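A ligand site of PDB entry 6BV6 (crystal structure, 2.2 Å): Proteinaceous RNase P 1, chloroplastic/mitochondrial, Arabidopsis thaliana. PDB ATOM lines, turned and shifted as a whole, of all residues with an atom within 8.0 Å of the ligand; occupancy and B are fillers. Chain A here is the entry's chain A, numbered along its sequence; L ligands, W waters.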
ATOM      1  N   ASN A 270      35.011 -15.667  27.961  1.00  0.00           N
ATOM      2  CA  ASN A 270      34.266 -15.958  26.713  1.00  0.00           C
ATOM      3  C   ASN A 270      33.454 -17.281  26.695  1.00  0.00           C
ATOM      4  O   ASN A 270      32.884 -17.626  25.678  1.00  0.00           O
ATOM      5  CB  ASN A 270      35.250 -15.982  25.541  1.00  0.00           C
ATOM      6  CG  ASN A 270      36.003 -14.671  25.407  1.00  0.00           C
ATOM      7  OD1 ASN A 270      37.140 -14.551  25.851  1.00  0.00           O
ATOM      8  ND2 ASN A 270      35.351 -13.687  24.799  1.00  0.00           N
ATOM      9  N   LYS A 279      33.804 -23.977  23.283  1.00  0.00           N
ATOM     10  CA  LYS A 279      33.107 -22.729  23.507  1.00  0.00           C
ATOM     11  C   LYS A 279      31.662 -23.082  23.828  1.00  0.00           C
ATOM     12  O   LYS A 279      30.982 -23.660  22.985  1.00  0.00           O
ATOM     13  CB  LYS A 279      33.168 -21.846  22.265  1.00  0.00           C
ATOM     14  CG  LYS A 279      32.687 -20.418  22.488  1.00  0.00           C
ATOM     15  CD  LYS A 279      32.714 -19.611  21.202  1.00  0.00           C
ATOM     16  CE  LYS A 279      31.913 -18.318  21.329  1.00  0.00           C
ATOM     17  NZ  LYS A 279      32.473 -17.415  22.363  1.00  0.00           N
ATOM     18  N   LEU A 280      31.209 -22.700  25.008  1.00  0.00           N
ATOM     19  CA  LEU A 280      29.862 -22.928  25.422  1.00  0.00           C
ATOM     20  C   LEU A 280      28.920 -22.038  24.653  1.00  0.00           C
ATOM     21  O   LEU A 280      29.277 -21.001  24.179  1.00  0.00           O
ATOM     22  CB  LEU A 280      29.684 -22.687  26.894  1.00  0.00           C
ATOM     23  CG  LEU A 280      30.366 -23.694  27.778  1.00  0.00           C
ATOM     24  CD1 LEU A 280      29.976 -23.427  29.195  1.00  0.00           C
ATOM     25  CD2 LEU A 280      30.034 -25.093  27.373  1.00  0.00           C
ATOM     26  N   VAL A 281      27.721 -22.519  24.529  1.00  0.00           N
ATOM     27  CA  VAL A 281      26.656 -21.867  23.819  1.00  0.00           C
ATOM     28  C   VAL A 281      25.908 -20.771  24.601  1.00  0.00           C
ATOM     29  O   VAL A 281      25.838 -20.798  25.792  1.00  0.00           O
ATOM     30  CB  VAL A 281      25.731 -22.966  23.243  1.00  0.00           C
ATOM     31  CG1 VAL A 281      24.355 -22.495  22.940  1.00  0.00           C
ATOM     32  CG2 VAL A 281      26.362 -23.556  22.015  1.00  0.00           C
ATOM     33  N   CYS A 282      25.378 -19.817  23.851  1.00  0.00           N
ATOM     34  CA  CYS A 282      24.550 -18.724  24.361  1.00  0.00           C
ATOM     35  C   CYS A 282      23.171 -19.030  23.828  1.00  0.00           C
ATOM     36  O   CYS A 282      22.955 -19.040  22.644  1.00  0.00           O
ATOM     37  CB  CYS A 282      25.006 -17.342  23.872  1.00  0.00           C
ATOM     38  SG  CYS A 282      24.342 -15.930  24.778  1.00  0.00           S
ATOM     39  N   ILE A 283      22.251 -19.254  24.734  1.00  0.00           N
ATOM     40  CA  ILE A 283      20.893 -19.647  24.429  1.00  0.00           C
ATOM     41  C   ILE A 283      19.903 -18.506  24.459  1.00  0.00           C
ATOM     42  O   ILE A 283      19.852 -17.782  25.394  1.00  0.00           O
ATOM     43  CB  ILE A 283      20.444 -20.720  25.418  1.00  0.00           C
ATOM     44  CG1 ILE A 283      21.425 -21.875  25.366  1.00  0.00           C
ATOM     45  CG2 ILE A 283      19.054 -21.169  25.128  1.00  0.00           C
ATOM     46  CD1 ILE A 283      21.227 -22.883  26.426  1.00  0.00           C
ATOM     47  N   ASP A 284      19.137 -18.387  23.395  1.00  0.00           N
ATOM     48  CA  ASP A 284      18.199 -17.289  23.241  1.00  0.00           C
ATOM     49  C   ASP A 284      17.036 -17.360  24.205  1.00  0.00           C
ATOM     50  O   ASP A 284      16.649 -18.418  24.669  1.00  0.00           O
ATOM     51  CB  ASP A 284      17.627 -17.284  21.816  1.00  0.00           C
ATOM     52  CG  ASP A 284      18.657 -16.941  20.753  1.00  0.00           C
ATOM     53  OD1 ASP A 284      19.723 -16.360  21.061  1.00  0.00           O
ATOM     54  OD2 ASP A 284      18.363 -17.247  19.573  1.00  0.00           O
ATOM     55  N   ILE A 285      16.475 -16.193  24.472  1.00  0.00           N
ATOM     56  CA  ILE A 285      15.218 -16.056  25.154  1.00  0.00           C
ATOM     57  C   ILE A 285      14.124 -15.784  24.096  1.00  0.00           C
ATOM     58  O   ILE A 285      14.283 -14.932  23.229  1.00  0.00           O
ATOM     59  CB  ILE A 285      15.294 -14.947  26.239  1.00  0.00           C
ATOM     60  CG1 ILE A 285      16.107 -15.484  27.424  1.00  0.00           C
ATOM     61  CG2 ILE A 285      13.908 -14.530  26.701  1.00  0.00           C
ATOM     62  CD1 ILE A 285      16.345 -14.476  28.527  1.00  0.00           C
ATOM     63  N   LEU A 417      19.554  -3.210  30.059  1.00  0.00           N
ATOM     64  CA  LEU A 417      20.322  -3.732  31.183  1.00  0.00           C
ATOM     65  C   LEU A 417      19.734  -3.278  32.529  1.00  0.00           C
ATOM     66  O   LEU A 417      19.164  -2.158  32.616  1.00  0.00           O
ATOM     67  CB  LEU A 417      21.749  -3.252  31.049  1.00  0.00           C
ATOM     68  CG  LEU A 417      22.474  -3.752  29.787  1.00  0.00           C
ATOM     69  CD1 LEU A 417      23.776  -2.980  29.617  1.00  0.00           C
ATOM     70  CD2 LEU A 417      22.735  -5.234  29.828  1.00  0.00           C
ATOM     71  N   ARG A 439      16.943 -16.910  33.804  1.00  0.00           N
ATOM     72  CA  ARG A 439      17.491 -16.741  32.431  1.00  0.00           C
ATOM     73  C   ARG A 439      17.510 -15.281  32.006  1.00  0.00           C
ATOM     74  O   ARG A 439      18.491 -14.827  31.393  1.00  0.00           O
ATOM     75  CB  ARG A 439      16.744 -17.613  31.399  1.00  0.00           C
ATOM     76  CG  ARG A 439      17.085 -19.118  31.480  1.00  0.00           C
ATOM     77  CD  ARG A 439      15.904 -20.030  31.178  1.00  0.00           C
ATOM     78  NE  ARG A 439      15.352 -19.652  29.904  1.00  0.00           N
ATOM     79  CZ  ARG A 439      14.075 -19.537  29.564  1.00  0.00           C
ATOM     80  NH1 ARG A 439      13.074 -19.830  30.387  1.00  0.00           N
ATOM     81  NH2 ARG A 439      13.813 -19.136  28.334  1.00  0.00           N
ATOM     82  N   GLU A 442      20.279 -13.346  33.985  1.00  0.00           N
ATOM     83  CA  GLU A 442      21.619 -13.626  33.470  1.00  0.00           C
ATOM     84  C   GLU A 442      21.934 -12.747  32.234  1.00  0.00           C
ATOM     85  O   GLU A 442      23.039 -12.199  32.111  1.00  0.00           O
ATOM     86  CB  GLU A 442      21.723 -15.104  33.133  1.00  0.00           C
ATOM     87  CG  GLU A 442      22.940 -15.515  32.353  1.00  0.00           C
ATOM     88  CD  GLU A 442      22.979 -17.035  32.143  1.00  0.00           C
ATOM     89  OE1 GLU A 442      22.339 -17.563  31.216  1.00  0.00           O
ATOM     90  OE2 GLU A 442      23.662 -17.709  32.901  1.00  0.00           O
ATOM     91  N   LYS A 443      20.978 -12.605  31.328  1.00  0.00           N
ATOM     92  CA  LYS A 443      21.154 -11.731  30.165  1.00  0.00           C
ATOM     93  C   LYS A 443      21.153 -10.254  30.448  1.00  0.00           C
ATOM     94  O   LYS A 443      21.713  -9.516  29.669  1.00  0.00           O
ATOM     95  CB  LYS A 443      20.147 -12.040  29.079  1.00  0.00           C
ATOM     96  CG  LYS A 443      20.292 -13.453  28.544  1.00  0.00           C
ATOM     97  CD  LYS A 443      19.764 -13.570  27.138  1.00  0.00           C
ATOM     98  CE  LYS A 443      19.776 -15.024  26.687  1.00  0.00           C
ATOM     99  NZ  LYS A 443      21.091 -15.439  26.148  1.00  0.00           N
ATOM    100  N   HIS A 444      20.505  -9.798  31.525  1.00  0.00           N
ATOM    101  CA  HIS A 444      20.227  -8.345  31.723  1.00  0.00           C
ATOM    102  C   HIS A 444      20.935  -7.692  32.889  1.00  0.00           C
ATOM    103  O   HIS A 444      21.113  -6.500  32.886  1.00  0.00           O
ATOM    104  CB  HIS A 444      18.701  -8.100  31.793  1.00  0.00           C
ATOM    105  CG  HIS A 444      18.007  -8.399  30.502  1.00  0.00           C
ATOM    106  ND1 HIS A 444      17.663  -7.405  29.601  1.00  0.00           N
ATOM    107  CD2 HIS A 444      17.661  -9.564  29.915  1.00  0.00           C
ATOM    108  CE1 HIS A 444      17.106  -7.954  28.535  1.00  0.00           C
ATOM    109  NE2 HIS A 444      17.096  -9.257  28.700  1.00  0.00           N
ATOM    110  N   MET A 460      29.495  -7.214  33.237  1.00  0.00           N
ATOM    111  CA  MET A 460      28.477  -7.368  32.211  1.00  0.00           C
ATOM    112  C   MET A 460      27.943  -8.773  32.156  1.00  0.00           C
ATOM    113  O   MET A 460      28.524  -9.677  32.729  1.00  0.00           O
ATOM    114  CB  MET A 460      29.033  -6.923  30.834  1.00  0.00           C
ATOM    115  CG  MET A 460      29.632  -5.511  30.821  1.00  0.00           C
ATOM    116  SD  MET A 460      28.472  -4.222  31.384  1.00  0.00           S
ATOM    117  CE  MET A 460      27.323  -4.194  30.004  1.00  0.00           C
ATOM    118  N   PRO A 461      26.782  -8.961  31.498  1.00  0.00           N
ATOM    119  CA  PRO A 461      26.241 -10.288  31.265  1.00  0.00           C
ATOM    120  C   PRO A 461      27.220 -11.148  30.457  1.00  0.00           C
ATOM    121  O   PRO A 461      27.862 -10.629  29.538  1.00  0.00           O
ATOM    122  CB  PRO A 461      24.995 -10.007  30.437  1.00  0.00           C
ATOM    123  CG  PRO A 461      24.533  -8.715  30.930  1.00  0.00           C
ATOM    124  CD  PRO A 461      25.807  -7.924  31.115  1.00  0.00           C
ATOM    125  N   PRO A 462      27.354 -12.439  30.809  1.00  0.00           N
ATOM    126  CA  PRO A 462      28.326 -13.250  30.071  1.00  0.00           C
ATOM    127  C   PRO A 462      27.876 -13.523  28.630  1.00  0.00           C
ATOM    128  O   PRO A 462      26.678 -13.601  28.363  1.00  0.00           O
ATOM    129  CB  PRO A 462      28.368 -14.543  30.880  1.00  0.00           C
ATOM    130  CG  PRO A 462      26.960 -14.650  31.380  1.00  0.00           C
ATOM    131  CD  PRO A 462      26.683 -13.255  31.844  1.00  0.00           C
ATOM    132  N   PRO A 463      28.833 -13.717  27.707  1.00  0.00           N
ATOM    133  CA  PRO A 463      28.515 -14.078  26.314  1.00  0.00           C
ATOM    134  C   PRO A 463      28.210 -15.578  26.092  1.00  0.00           C
ATOM    135  O   PRO A 463      28.468 -16.092  25.017  1.00  0.00           O
ATOM    136  CB  PRO A 463      29.779 -13.656  25.542  1.00  0.00           C
ATOM    137  CG  PRO A 463      30.884 -13.765  26.531  1.00  0.00           C
ATOM    138  CD  PRO A 463      30.277 -13.523  27.899  1.00  0.00           C
ATOM    139  N   TYR A 464      27.650 -16.233  27.103  1.00  0.00           N
ATOM    140  CA  TYR A 464      27.267 -17.633  27.032  1.00  0.00           C
ATOM    141  C   TYR A 464      26.267 -17.878  28.163  1.00  0.00           C
ATOM    142  O   TYR A 464      26.120 -17.047  29.047  1.00  0.00           O
ATOM    143  CB  TYR A 464      28.508 -18.524  27.138  1.00  0.00           C
ATOM    144  CG  TYR A 464      29.226 -18.467  28.478  1.00  0.00           C
ATOM    145  CD1 TYR A 464      30.087 -17.429  28.792  1.00  0.00           C
ATOM    146  CD2 TYR A 464      29.048 -19.467  29.409  1.00  0.00           C
ATOM    147  CE1 TYR A 464      30.735 -17.391  30.016  1.00  0.00           C
ATOM    148  CE2 TYR A 464      29.700 -19.450  30.626  1.00  0.00           C
ATOM    149  CZ  TYR A 464      30.524 -18.405  30.943  1.00  0.00           C
ATOM    150  OH  TYR A 464      31.145 -18.430  32.191  1.00  0.00           O
ATOM    151  N   SER A 465      25.554 -18.990  28.105  1.00  0.00           N
ATOM    152  CA  SER A 465      24.570 -19.320  29.130  1.00  0.00           C
ATOM    153  C   SER A 465      25.180 -20.256  30.135  1.00  0.00           C
ATOM    154  O   SER A 465      25.723 -21.330  29.766  1.00  0.00           O
ATOM    155  CB  SER A 465      23.332 -19.960  28.526  1.00  0.00           C
ATOM    156  OG  SER A 465      22.830 -19.097  27.554  1.00  0.00           O
HETATM  157  O1  LIG L   1      27.449 -13.249  22.174  1.00  0.00           O
HETATM  158  C1  LIG L   1      26.522 -13.261  23.174  1.00  0.00           C
HETATM  159  C2  LIG L   1      25.870 -14.455  23.493  1.00  0.00           C
HETATM  160  C3  LIG L   1      24.932 -14.502  24.511  1.00  0.00           C
HETATM  161  C4  LIG L   1      24.634 -13.320  25.212  1.00  0.00           C
HETATM  162  O2  LIG L   1      23.707 -13.403  26.212  1.00  0.00           O
HETATM  163  C5  LIG L   1      25.257 -12.084  24.924  1.00  0.00           C
HETATM  164  C6  LIG L   1      26.234 -12.066  23.880  1.00  0.00           C
HETATM  165  C7  LIG L   1      26.901 -10.872  23.536  1.00  0.00           C
HETATM  166  C8  LIG L   1      26.600  -9.698  24.243  1.00  0.00           C
HETATM  167  C9  LIG L   1      25.660  -9.696  25.285  1.00  0.00           C
HETATM  168  C10 LIG L   1      24.984 -10.889  25.623  1.00  0.00           C
HETATM  169  O3  LIG L   1      24.048 -10.908  26.658  1.00  0.00           O
HETATM  170  O   HOH W   1      23.935 -14.507  29.047  1.00  0.00           O
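SG of Cys 282 is covalently linked to C3 of the ligand, 1.6 Å away.
NZ of Lys 443 lies within hydrogen-bond range of O2 of the ligand.
The side-chain amino group (NZ) of Lys 443 lies within hydrogen-bond range of the side-chain sulfur (SG) of Cys 282, 3.6 Å away.
NZ of Lys 443 lies within hydrogen-bond range of O of Ile 283.
Residues that only touch the ligand: Pro 461, Pro 462 and Pro 463.
Of the 19 residues printed, 5 come within 4 Å of the ligand.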
